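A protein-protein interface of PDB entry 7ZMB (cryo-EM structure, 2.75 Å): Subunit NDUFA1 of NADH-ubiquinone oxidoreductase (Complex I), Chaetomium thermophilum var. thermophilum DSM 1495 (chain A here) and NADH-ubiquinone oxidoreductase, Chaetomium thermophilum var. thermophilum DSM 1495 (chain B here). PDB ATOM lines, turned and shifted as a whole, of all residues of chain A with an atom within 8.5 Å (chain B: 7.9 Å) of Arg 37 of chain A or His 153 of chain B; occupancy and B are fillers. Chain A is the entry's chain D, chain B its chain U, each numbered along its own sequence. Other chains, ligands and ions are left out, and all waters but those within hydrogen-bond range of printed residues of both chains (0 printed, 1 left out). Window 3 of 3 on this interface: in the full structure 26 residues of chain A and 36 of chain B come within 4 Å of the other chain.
NE of Arg 39 of chain A sits at hydrogen-bond distance from OD1 of Asn 106 of chain B (3.0 Å). The side-chain amino group (NZ) of Lys 36 of chain A is in salt-bridge range of the side-chain carboxylate (OD2) of Asp 103 of chain B (2.8 Å). The guanidinium group (NH1) of Arg 61 of chain A lies within salt-bridge range of the side-chain carboxylate (OD1) of Asp 103 of chain B (3.4 Å). N of Trp 40 of chain A lies within hydrogen-bond range of OD1 of Asn 106 of chain B. O of Asn 104 of chain B lies within hydrogen-bond range of NE of Arg 37 of chain A (2.9 Å).
ND1 of His 153 of chain B sits at hydrogen-bond distance from ND1 of His 154 of chain B. The side-chain amide oxygen of Asn 33 of chain A lies within hydrogen-bond range of the guanidinium group of Arg 61 of chain A (3.3 Å). O of His 30 of chain A lies within hydrogen-bond range of N of Lys 36 of chain A (3.1 Å). O of Arg 37 of chain A sits at hydrogen-bond distance from NH2 of Arg 61 of chain A, 2.9 Å away. The side-chain amide oxygen (OD1) of Asn 105 of chain B sits close to the backbone carbonyl oxygen (O) of Gln 111 of chain B, at 3.3 Å. The side-chain amide nitrogen (ND2) of Asn 106 of chain B sits at hydrogen-bond distance from the side-chain amide oxygen (OE1) of Gln 108 of chain B, at 2.9 Å.
Lys 36 of chain A touches Asn 104 of chain B (NZ to OD1, 3.96 Å). Arg 37 of chain A touches Asn 105 of chain B. NH1 of Arg 37 of chain A touches NE2 of His 153 of chain B (3.6 Å). NE1 of Trp 40 of chain A touches OE1 of Gln 108 of chain B, at 3.7 Å.
Of chain B, only Asn 104, Asn 105 and His 153 come within 4 Å of Arg 37 of chain A. Of chain A, only Arg 37 (3.6 Å) comes within 4 Å of His 153 of chain B. Printed residues of chain A within 4 Å of Asn 105 of chain B: Arg 37 (3.6 Å). Printed residues of chain B within 4 Å of Arg 61 of chain A: Asp 103. Gly 34 of chain A touches none of the printed residues of chain B. Phe 32 of chain A touches none of the printed residues of chain B. The nearest printed residue of chain A that does not touch Asn 104 of chain B is Arg 61 of chain A (5.1 Å).
Printed residues of chain B that touch a printed residue of chain A: Asp 103, Asn 104, Asn 105, Asn 106, Gln 108 and His 153. Hydrophobic or aromatic side chains of chain A that line the printed part of chain B: Trp 40. Among the printed residues, 9 pairs touch across the chains. Among the printed residues, Asp or Glu carboxylates within 4 Å of a Lys or Arg side-chain nitrogen of the other chain: Lys 36 of chain A with Asp 103 of chain B and Arg 61 of chain A with Asp 103 of chain B.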
ATOM      1  N   ALA A  26     -11.354 -18.201   4.274  1.00  0.00           N
ATOM      2  CA  ALA A  26     -10.282 -17.743   3.402  1.00  0.00           C
ATOM      3  C   ALA A  26      -8.919 -17.881   4.069  1.00  0.00           C
ATOM      4  O   ALA A  26      -7.948 -18.285   3.425  1.00  0.00           O
ATOM      5  CB  ALA A  26     -10.542 -16.299   2.983  1.00  0.00           C
ATOM      6  N   ARG A  29      -7.765 -21.651   4.351  1.00  0.00           N
ATOM      7  CA  ARG A  29      -7.400 -22.279   3.063  1.00  0.00           C
ATOM      8  C   ARG A  29      -6.218 -21.531   2.455  1.00  0.00           C
ATOM      9  O   ARG A  29      -5.517 -22.141   1.653  1.00  0.00           O
ATOM     10  CB  ARG A  29      -8.610 -22.518   2.142  1.00  0.00           C
ATOM     11  CG  ARG A  29      -9.229 -23.894   2.312  1.00  0.00           C
ATOM     12  CD  ARG A  29      -9.648 -24.658   1.073  1.00  0.00           C
ATOM     13  NE  ARG A  29     -10.490 -23.918   0.146  1.00  0.00           N
ATOM     14  CZ  ARG A  29     -11.811 -23.829   0.208  1.00  0.00           C
ATOM     15  NH1 ARG A  29     -12.457 -23.131  -0.705  1.00  0.00           N
ATOM     16  NH2 ARG A  29     -12.483 -24.415   1.182  1.00  0.00           N
ATOM     17  N   HIS A  30      -5.999 -20.279   2.859  1.00  0.00           N
ATOM     18  CA  HIS A  30      -4.833 -19.519   2.340  1.00  0.00           C
ATOM     19  C   HIS A  30      -3.654 -20.117   3.083  1.00  0.00           C
ATOM     20  O   HIS A  30      -2.610 -20.289   2.461  1.00  0.00           O
ATOM     21  CB  HIS A  30      -5.027 -18.006   2.492  1.00  0.00           C
ATOM     22  CG  HIS A  30      -3.887 -17.181   1.998  1.00  0.00           C
ATOM     23  ND1 HIS A  30      -2.816 -16.851   2.801  1.00  0.00           N
ATOM     24  CD2 HIS A  30      -3.666 -16.588   0.807  1.00  0.00           C
ATOM     25  CE1 HIS A  30      -1.980 -16.094   2.123  1.00  0.00           C
ATOM     26  NE2 HIS A  30      -2.473 -15.926   0.895  1.00  0.00           N
ATOM     27  N   MET A  31      -3.835 -20.480   4.351  1.00  0.00           N
ATOM     28  CA  MET A  31      -2.836 -21.238   5.100  1.00  0.00           C
ATOM     29  C   MET A  31      -2.642 -22.634   4.527  1.00  0.00           C
ATOM     30  O   MET A  31      -1.508 -23.101   4.386  1.00  0.00           O
ATOM     31  CB  MET A  31      -3.248 -21.335   6.568  1.00  0.00           C
ATOM     32  CG  MET A  31      -2.222 -22.006   7.457  1.00  0.00           C
ATOM     33  SD  MET A  31      -0.669 -21.095   7.552  1.00  0.00           S
ATOM     34  CE  MET A  31      -1.157 -19.701   8.562  1.00  0.00           C
ATOM     35  N   PHE A  32      -3.721 -23.340   4.210  1.00  0.00           N
ATOM     36  CA  PHE A  32      -3.610 -24.749   3.744  1.00  0.00           C
ATOM     37  C   PHE A  32      -2.926 -24.850   2.373  1.00  0.00           C
ATOM     38  O   PHE A  32      -2.335 -25.901   2.084  1.00  0.00           O
ATOM     39  CB  PHE A  32      -5.016 -25.323   3.605  1.00  0.00           C
ATOM     40  CG  PHE A  32      -5.114 -26.820   3.715  1.00  0.00           C
ATOM     41  CD1 PHE A  32      -4.423 -27.498   4.704  1.00  0.00           C
ATOM     42  CD2 PHE A  32      -5.907 -27.543   2.843  1.00  0.00           C
ATOM     43  CE1 PHE A  32      -4.519 -28.873   4.818  1.00  0.00           C
ATOM     44  CE2 PHE A  32      -6.004 -28.920   2.959  1.00  0.00           C
ATOM     45  CZ  PHE A  32      -5.310 -29.579   3.946  1.00  0.00           C
ATOM     46  N   ASN A  33      -2.982 -23.800   1.553  1.00  0.00           N
ATOM     47  CA  ASN A  33      -2.471 -23.872   0.161  1.00  0.00           C
ATOM     48  C   ASN A  33      -1.067 -23.286   0.078  1.00  0.00           C
ATOM     49  O   ASN A  33      -0.546 -23.191  -1.043  1.00  0.00           O
ATOM     50  CB  ASN A  33      -3.491 -23.320  -0.834  1.00  0.00           C
ATOM     51  CG  ASN A  33      -4.660 -24.256  -1.058  1.00  0.00           C
ATOM     52  OD1 ASN A  33      -4.614 -25.108  -1.939  1.00  0.00           O
ATOM     53  ND2 ASN A  33      -5.706 -24.117  -0.261  1.00  0.00           N
ATOM     54  N   GLY A  34      -0.476 -22.929   1.207  1.00  0.00           N
ATOM     55  CA  GLY A  34       0.923 -22.475   1.237  1.00  0.00           C
ATOM     56  C   GLY A  34       0.989 -20.976   1.134  1.00  0.00           C
ATOM     57  O   GLY A  34       1.721 -20.484   0.261  1.00  0.00           O
ATOM     58  N   ASP A  35       0.287 -20.286   2.034  1.00  0.00           N
ATOM     59  CA  ASP A  35       0.181 -18.830   1.998  1.00  0.00           C
ATOM     60  C   ASP A  35      -0.236 -18.357   0.611  1.00  0.00           C
ATOM     61  O   ASP A  35       0.224 -17.328   0.114  1.00  0.00           O
ATOM     62  CB  ASP A  35       1.487 -18.167   2.438  1.00  0.00           C
ATOM     63  CG  ASP A  35       1.967 -18.659   3.790  1.00  0.00           C
ATOM     64  OD1 ASP A  35       1.114 -19.030   4.626  1.00  0.00           O
ATOM     65  OD2 ASP A  35       3.194 -18.677   4.018  1.00  0.00           O
ATOM     66  N   LYS A  36      -1.123 -19.118  -0.019  1.00  0.00           N
ATOM     67  CA  LYS A  36      -1.542 -18.858  -1.385  1.00  0.00           C
ATOM     68  C   LYS A  36      -3.050 -19.007  -1.475  1.00  0.00           C
ATOM     69  O   LYS A  36      -3.653 -19.791  -0.739  1.00  0.00           O
ATOM     70  CB  LYS A  36      -0.868 -19.816  -2.373  1.00  0.00           C
ATOM     71  CG  LYS A  36       0.624 -19.604  -2.534  1.00  0.00           C
ATOM     72  CD  LYS A  36       1.281 -20.822  -3.162  1.00  0.00           C
ATOM     73  CE  LYS A  36       2.555 -20.454  -3.898  1.00  0.00           C
ATOM     74  NZ  LYS A  36       2.327 -19.374  -4.896  1.00  0.00           N
ATOM     75  N   ARG A  37      -3.654 -18.214  -2.364  1.00  0.00           N
ATOM     76  CA  ARG A  37      -5.122 -18.303  -2.549  1.00  0.00           C
ATOM     77  C   ARG A  37      -5.430 -19.698  -3.089  1.00  0.00           C
ATOM     78  O   ARG A  37      -4.620 -20.219  -3.869  1.00  0.00           O
ATOM     79  CB  ARG A  37      -5.683 -17.130  -3.359  1.00  0.00           C
ATOM     80  CG  ARG A  37      -7.160 -17.255  -3.696  1.00  0.00           C
ATOM     81  CD  ARG A  37      -7.908 -15.942  -3.850  1.00  0.00           C
ATOM     82  NE  ARG A  37      -7.434 -15.096  -4.934  1.00  0.00           N
ATOM     83  CZ  ARG A  37      -6.783 -13.949  -4.771  1.00  0.00           C
ATOM     84  NH1 ARG A  37      -6.392 -13.256  -5.827  1.00  0.00           N
ATOM     85  NH2 ARG A  37      -6.527 -13.497  -3.556  1.00  0.00           N
ATOM     86  N   HIS A  38      -6.534 -20.286  -2.652  1.00  0.00           N
ATOM     87  CA  HIS A  38      -6.916 -21.668  -3.035  1.00  0.00           C
ATOM     88  C   HIS A  38      -7.378 -21.744  -4.489  1.00  0.00           C
ATOM     89  O   HIS A  38      -7.316 -20.734  -5.182  1.00  0.00           O
ATOM     90  CB  HIS A  38      -8.039 -22.084  -2.093  1.00  0.00           C
ATOM     91  CG  HIS A  38      -9.259 -21.245  -2.277  1.00  0.00           C
ATOM     92  ND1 HIS A  38      -9.340 -19.946  -1.818  1.00  0.00           N
ATOM     93  CD2 HIS A  38     -10.427 -21.495  -2.903  1.00  0.00           C
ATOM     94  CE1 HIS A  38     -10.503 -19.434  -2.146  1.00  0.00           C
ATOM     95  NE2 HIS A  38     -11.190 -20.369  -2.802  1.00  0.00           N
ATOM     96  N   ARG A  39      -7.790 -22.927  -4.921  1.00  0.00           N
ATOM     97  CA  ARG A  39      -8.345 -23.109  -6.279  1.00  0.00           C
ATOM     98  C   ARG A  39      -9.831 -23.436  -6.195  1.00  0.00           C
ATOM     99  O   ARG A  39     -10.222 -24.088  -5.241  1.00  0.00           O
ATOM    100  CB  ARG A  39      -7.616 -24.271  -6.947  1.00  0.00           C
ATOM    101  CG  ARG A  39      -6.112 -24.077  -7.061  1.00  0.00           C
ATOM    102  CD  ARG A  39      -5.802 -22.939  -8.006  1.00  0.00           C
ATOM    103  NE  ARG A  39      -6.352 -23.196  -9.325  1.00  0.00           N
ATOM    104  CZ  ARG A  39      -5.731 -23.890 -10.268  1.00  0.00           C
ATOM    105  NH1 ARG A  39      -4.539 -24.403 -10.030  1.00  0.00           N
ATOM    106  NH2 ARG A  39      -6.306 -24.072 -11.442  1.00  0.00           N
ATOM    107  N   TRP A  40     -10.625 -22.985  -7.156  1.00  0.00           N
ATOM    108  CA  TRP A  40     -12.069 -23.310  -7.229  1.00  0.00           C
ATOM    109  C   TRP A  40     -12.445 -23.672  -8.665  1.00  0.00           C
ATOM    110  O   TRP A  40     -11.641 -23.374  -9.560  1.00  0.00           O
ATOM    111  CB  TRP A  40     -12.923 -22.152  -6.706  1.00  0.00           C
ATOM    112  CG  TRP A  40     -12.787 -20.855  -7.438  1.00  0.00           C
ATOM    113  CD1 TRP A  40     -13.555 -20.414  -8.474  1.00  0.00           C
ATOM    114  CD2 TRP A  40     -11.846 -19.802  -7.161  1.00  0.00           C
ATOM    115  NE1 TRP A  40     -13.148 -19.172  -8.872  1.00  0.00           N
ATOM    116  CE2 TRP A  40     -12.100 -18.770  -8.088  1.00  0.00           C
ATOM    117  CE3 TRP A  40     -10.810 -19.637  -6.237  1.00  0.00           C
ATOM    118  CZ2 TRP A  40     -11.358 -17.590  -8.111  1.00  0.00           C
ATOM    119  CZ3 TRP A  40     -10.079 -18.471  -6.259  1.00  0.00           C
ATOM    120  CH2 TRP A  40     -10.352 -17.461  -7.183  1.00  0.00           C
ATOM    121  N   ARG A  61       0.508 -27.444  -4.627  1.00  0.00           N
ATOM    122  CA  ARG A  61       0.317 -26.046  -5.077  1.00  0.00           C
ATOM    123  C   ARG A  61       1.656 -25.309  -5.191  1.00  0.00           C
ATOM    124  O   ARG A  61       1.636 -24.074  -5.140  1.00  0.00           O
ATOM    125  CB  ARG A  61      -0.662 -25.403  -4.094  1.00  0.00           C
ATOM    126  CG  ARG A  61      -2.106 -25.856  -4.242  1.00  0.00           C
ATOM    127  CD  ARG A  61      -2.754 -25.249  -5.469  1.00  0.00           C
ATOM    128  NE  ARG A  61      -2.340 -23.876  -5.720  1.00  0.00           N
ATOM    129  CZ  ARG A  61      -2.919 -22.807  -5.194  1.00  0.00           C
ATOM    130  NH1 ARG A  61      -2.471 -21.599  -5.483  1.00  0.00           N
ATOM    131  NH2 ARG A  61      -3.943 -22.949  -4.372  1.00  0.00           N
ATOM    132  N   CYS B 101       1.146 -14.200 -10.220  1.00  0.00           N
ATOM    133  CA  CYS B 101      -0.206 -13.606 -10.110  1.00  0.00           C
ATOM    134  C   CYS B 101      -1.189 -14.718 -10.468  1.00  0.00           C
ATOM    135  O   CYS B 101      -2.196 -14.853  -9.769  1.00  0.00           O
ATOM    136  CB  CYS B 101      -0.368 -12.391 -11.015  1.00  0.00           C
ATOM    137  SG  CYS B 101      -2.079 -11.816 -11.162  1.00  0.00           S
ATOM    138  N   LEU B 102      -0.873 -15.490 -11.518  1.00  0.00           N
ATOM    139  CA  LEU B 102      -1.768 -16.564 -12.013  1.00  0.00           C
ATOM    140  C   LEU B 102      -1.979 -17.597 -10.915  1.00  0.00           C
ATOM    141  O   LEU B 102      -3.097 -18.100 -10.799  1.00  0.00           O
ATOM    142  CB  LEU B 102      -1.111 -17.206 -13.237  1.00  0.00           C
ATOM    143  CG  LEU B 102      -1.310 -16.473 -14.561  1.00  0.00           C
ATOM    144  CD1 LEU B 102      -0.486 -17.123 -15.658  1.00  0.00           C
ATOM    145  CD2 LEU B 102      -2.781 -16.441 -14.947  1.00  0.00           C
ATOM    146  N   ASP B 103      -0.932 -17.901 -10.154  1.00  0.00           N
ATOM    147  CA  ASP B 103      -1.033 -18.893  -9.053  1.00  0.00           C
ATOM    148  C   ASP B 103      -1.982 -18.392  -7.975  1.00  0.00           C
ATOM    149  O   ASP B 103      -2.644 -19.223  -7.364  1.00  0.00           O
ATOM    150  CB  ASP B 103       0.327 -19.279  -8.468  1.00  0.00           C
ATOM    151  CG  ASP B 103       0.266 -20.642  -7.803  1.00  0.00           C
ATOM    152  OD1 ASP B 103      -0.490 -21.500  -8.302  1.00  0.00           O
ATOM    153  OD2 ASP B 103       0.942 -20.827  -6.783  1.00  0.00           O
ATOM    154  N   ASN B 104      -1.967 -17.088  -7.703  1.00  0.00           N
ATOM    155  CA  ASN B 104      -2.852 -16.497  -6.671  1.00  0.00           C
ATOM    156  C   ASN B 104      -4.239 -16.243  -7.246  1.00  0.00           C
ATOM    157  O   ASN B 104      -5.124 -15.951  -6.447  1.00  0.00           O
ATOM    158  CB  ASN B 104      -2.258 -15.222  -6.074  1.00  0.00           C
ATOM    159  CG  ASN B 104      -0.960 -15.451  -5.332  1.00  0.00           C
ATOM    160  OD1 ASN B 104      -0.428 -16.559  -5.317  1.00  0.00           O
ATOM    161  ND2 ASN B 104      -0.440 -14.403  -4.717  1.00  0.00           N
ATOM    162  N   ASN B 105      -4.436 -16.388  -8.561  1.00  0.00           N
ATOM    163  CA  ASN B 105      -5.736 -15.995  -9.178  1.00  0.00           C
ATOM    164  C   ASN B 105      -6.522 -17.152  -9.807  1.00  0.00           C
ATOM    165  O   ASN B 105      -7.346 -16.853 -10.669  1.00  0.00           O
ATOM    166  CB  ASN B 105      -5.565 -14.835 -10.158  1.00  0.00           C
ATOM    167  CG  ASN B 105      -5.313 -13.496  -9.492  1.00  0.00           C
ATOM    168  OD1 ASN B 105      -6.080 -12.558  -9.670  1.00  0.00           O
ATOM    169  ND2 ASN B 105      -4.238 -13.384  -8.734  1.00  0.00           N
ATOM    170  N   ASN B 106      -6.278 -18.403  -9.414  1.00  0.00           N
ATOM    171  CA  ASN B 106      -7.050 -19.579  -9.908  1.00  0.00           C
ATOM    172  C   ASN B 106      -6.651 -19.876 -11.359  1.00  0.00           C
ATOM    173  O   ASN B 106      -7.469 -20.454 -12.098  1.00  0.00           O
ATOM    174  CB  ASN B 106      -8.545 -19.455  -9.583  1.00  0.00           C
ATOM    175  CG  ASN B 106      -9.342 -20.731  -9.747  1.00  0.00           C
ATOM    176  OD1 ASN B 106      -8.947 -21.786  -9.267  1.00  0.00           O
ATOM    177  ND2 ASN B 106     -10.481 -20.640 -10.412  1.00  0.00           N
ATOM    178  N   GLN B 108      -6.583 -18.001 -13.728  1.00  0.00           N
ATOM    179  CA  GLN B 108      -7.496 -17.292 -14.657  1.00  0.00           C
ATOM    180  C   GLN B 108      -6.713 -16.165 -15.327  1.00  0.00           C
ATOM    181  O   GLN B 108      -6.184 -15.314 -14.606  1.00  0.00           O
ATOM    182  CB  GLN B 108      -8.769 -16.878 -13.919  1.00  0.00           C
ATOM    183  CG  GLN B 108      -9.524 -18.073 -13.351  1.00  0.00           C
ATOM    184  CD  GLN B 108     -10.704 -17.709 -12.486  1.00  0.00           C
ATOM    185  OE1 GLN B 108     -11.499 -18.563 -12.103  1.00  0.00           O
ATOM    186  NE2 GLN B 108     -10.833 -16.432 -12.176  1.00  0.00           N
ATOM    187  N   TRP B 110      -7.667 -13.635 -17.254  1.00  0.00           N
ATOM    188  CA  TRP B 110      -8.311 -12.300 -17.156  1.00  0.00           C
ATOM    189  C   TRP B 110      -7.994 -11.647 -15.809  1.00  0.00           C
ATOM    190  O   TRP B 110      -8.194 -10.437 -15.693  1.00  0.00           O
ATOM    191  CB  TRP B 110      -9.816 -12.388 -17.426  1.00  0.00           C
ATOM    192  CG  TRP B 110     -10.605 -13.225 -16.469  1.00  0.00           C
ATOM    193  CD1 TRP B 110     -11.243 -12.807 -15.339  1.00  0.00           C
ATOM    194  CD2 TRP B 110     -10.885 -14.630 -16.592  1.00  0.00           C
ATOM    195  NE1 TRP B 110     -11.886 -13.856 -14.741  1.00  0.00           N
ATOM    196  CE2 TRP B 110     -11.688 -14.985 -15.489  1.00  0.00           C
ATOM    197  CE3 TRP B 110     -10.537 -15.615 -17.520  1.00  0.00           C
ATOM    198  CZ2 TRP B 110     -12.138 -16.288 -15.292  1.00  0.00           C
ATOM    199  CZ3 TRP B 110     -10.985 -16.899 -17.324  1.00  0.00           C
ATOM    200  CH2 TRP B 110     -11.772 -17.230 -16.223  1.00  0.00           C
ATOM    201  N   GLN B 111      -7.574 -12.429 -14.820  1.00  0.00           N
ATOM    202  CA  GLN B 111      -7.342 -11.898 -13.456  1.00  0.00           C
ATOM    203  C   GLN B 111      -5.933 -11.305 -13.323  1.00  0.00           C
ATOM    204  O   GLN B 111      -5.665 -10.673 -12.298  1.00  0.00           O
ATOM    205  CB  GLN B 111      -7.594 -13.026 -12.455  1.00  0.00           C
ATOM    206  CG  GLN B 111      -9.015 -13.553 -12.451  1.00  0.00           C
ATOM    207  CD  GLN B 111      -9.948 -12.605 -11.744  1.00  0.00           C
ATOM    208  OE1 GLN B 111      -9.574 -11.490 -11.396  1.00  0.00           O
ATOM    209  NE2 GLN B 111     -11.175 -13.047 -11.525  1.00  0.00           N
ATOM    210  N   CYS B 112      -5.080 -11.491 -14.330  1.00  0.00           N
ATOM    211  CA  CYS B 112      -3.673 -11.009 -14.257  1.00  0.00           C
ATOM    212  C   CYS B 112      -3.294 -10.235 -15.521  1.00  0.00           C
ATOM    213  O   CYS B 112      -2.124 -10.317 -15.915  1.00  0.00           O
ATOM    214  CB  CYS B 112      -2.732 -12.195 -14.089  1.00  0.00           C
ATOM    215  SG  CYS B 112      -2.957 -13.060 -12.522  1.00  0.00           S
ATOM    216  N   GLN B 149     -11.719  -5.610 -17.832  1.00  0.00           N
ATOM    217  CA  GLN B 149     -12.105  -7.038 -17.756  1.00  0.00           C
ATOM    218  C   GLN B 149     -13.324  -7.152 -16.844  1.00  0.00           C
ATOM    219  O   GLN B 149     -13.187  -6.831 -15.665  1.00  0.00           O
ATOM    220  CB  GLN B 149     -10.931  -7.944 -17.391  1.00  0.00           C
ATOM    221  CG  GLN B 149      -9.818  -7.955 -18.426  1.00  0.00           C
ATOM    222  CD  GLN B 149     -10.231  -8.441 -19.794  1.00  0.00           C
ATOM    223  OE1 GLN B 149     -11.012  -9.377 -19.946  1.00  0.00           O
ATOM    224  NE2 GLN B 149      -9.670  -7.818 -20.814  1.00  0.00           N
ATOM    225  N   ILE B 150     -14.447  -7.659 -17.354  1.00  0.00           N
ATOM    226  CA  ILE B 150     -15.704  -7.684 -16.547  1.00  0.00           C
ATOM    227  C   ILE B 150     -15.649  -8.786 -15.483  1.00  0.00           C
ATOM    228  O   ILE B 150     -16.311  -8.611 -14.439  1.00  0.00           O
ATOM    229  CB  ILE B 150     -16.883  -7.973 -17.503  1.00  0.00           C
ATOM    230  CG1 ILE B 150     -17.037  -6.910 -18.593  1.00  0.00           C
ATOM    231  CG2 ILE B 150     -18.188  -8.189 -16.750  1.00  0.00           C
ATOM    232  CD1 ILE B 150     -18.122  -7.229 -19.594  1.00  0.00           C
ATOM    233  N   PHE B 151     -14.821  -9.815 -15.664  1.00  0.00           N
ATOM    234  CA  PHE B 151     -14.839 -10.942 -14.697  1.00  0.00           C
ATOM    235  C   PHE B 151     -13.656 -10.841 -13.730  1.00  0.00           C
ATOM    236  O   PHE B 151     -13.526 -11.717 -12.862  1.00  0.00           O
ATOM    237  CB  PHE B 151     -15.057 -12.271 -15.424  1.00  0.00           C
ATOM    238  CG  PHE B 151     -16.409 -12.383 -16.077  1.00  0.00           C
ATOM    239  CD1 PHE B 151     -17.532 -12.697 -15.329  1.00  0.00           C
ATOM    240  CD2 PHE B 151     -16.565 -12.150 -17.432  1.00  0.00           C
ATOM    241  CE1 PHE B 151     -18.780 -12.788 -15.926  1.00  0.00           C
ATOM    242  CE2 PHE B 151     -17.813 -12.237 -18.026  1.00  0.00           C
ATOM    243  CZ  PHE B 151     -18.916 -12.557 -17.273  1.00  0.00           C
ATOM    244  N   ALA B 152     -12.857  -9.778 -13.850  1.00  0.00           N
ATOM    245  CA  ALA B 152     -11.692  -9.568 -12.956  1.00  0.00           C
ATOM    246  C   ALA B 152     -12.172  -9.025 -11.610  1.00  0.00           C
ATOM    247  O   ALA B 152     -12.952  -8.062 -11.618  1.00  0.00           O
ATOM    248  CB  ALA B 152     -10.720  -8.617 -13.587  1.00  0.00           C
ATOM    249  N   HIS B 153     -11.719  -9.626 -10.507  1.00  0.00           N
ATOM    250  CA  HIS B 153     -12.112  -9.125  -9.161  1.00  0.00           C
ATOM    251  C   HIS B 153     -11.513  -7.746  -8.895  1.00  0.00           C
ATOM    252  O   HIS B 153     -12.222  -6.904  -8.343  1.00  0.00           O
ATOM    253  CB  HIS B 153     -11.868 -10.160  -8.064  1.00  0.00           C
ATOM    254  CG  HIS B 153     -10.547 -10.836  -8.090  1.00  0.00           C
ATOM    255  ND1 HIS B 153      -9.380 -10.181  -7.779  1.00  0.00           N
ATOM    256  CD2 HIS B 153     -10.218 -12.120  -8.327  1.00  0.00           C
ATOM    257  CE1 HIS B 153      -8.376 -11.025  -7.856  1.00  0.00           C
ATOM    258  NE2 HIS B 153      -8.866 -12.221  -8.192  1.00  0.00           N
ATOM    259  N   HIS B 154     -10.237  -7.556  -9.232  1.00  0.00           N
ATOM    260  CA  HIS B 154      -9.613  -6.217  -9.101  1.00  0.00           C
ATOM    261  C   HIS B 154      -9.614  -5.557 -10.471  1.00  0.00           C
ATOM    262  O   HIS B 154      -9.079  -6.160 -11.418  1.00  0.00           O
ATOM    263  CB  HIS B 154      -8.216  -6.303  -8.491  1.00  0.00           C
ATOM    264  CG  HIS B 154      -8.226  -6.489  -7.013  1.00  0.00           C
ATOM    265  ND1 HIS B 154      -8.360  -7.732  -6.425  1.00  0.00           N
ATOM    266  CD2 HIS B 154      -8.124  -5.600  -6.001  1.00  0.00           C
ATOM    267  CE1 HIS B 154      -8.337  -7.602  -5.114  1.00  0.00           C
ATOM    268  NE2 HIS B 154      -8.193  -6.302  -4.829  1.00  0.00           N
ATOM    269  N   ALA B 155     -10.205  -4.372 -10.562  1.00  0.00           N
ATOM    270  CA  ALA B 155     -10.335  -3.671 -11.854  1.00  0.00           C
ATOM    271  C   ALA B 155      -8.967  -3.359 -12.442  1.00  0.00           C
ATOM    272  O   ALA B 155      -8.078  -2.959 -11.690  1.00  0.00           O
ATOM    273  CB  ALA B 155     -11.135  -2.417 -11.664  1.00  0.00           C
ATOM    274  N   ILE B 156      -8.839  -3.530 -13.762  1.00  0.00           N
ATOM    275  CA  ILE B 156      -7.552  -3.241 -14.451  1.00  0.00           C
ATOM    276  C   ILE B 156      -7.294  -1.754 -14.243  1.00  0.00           C
ATOM    277  O   ILE B 156      -8.220  -0.960 -14.436  1.00  0.00           O
ATOM    278  CB  ILE B 156      -7.594  -3.651 -15.944  1.00  0.00           C
ATOM    279  CG1 ILE B 156      -7.399  -5.156 -16.127  1.00  0.00           C
ATOM    280  CG2 ILE B 156      -6.568  -2.873 -16.753  1.00  0.00           C
ATOM    281  CD1 ILE B 156      -8.562  -5.983 -15.664  1.00  0.00           C
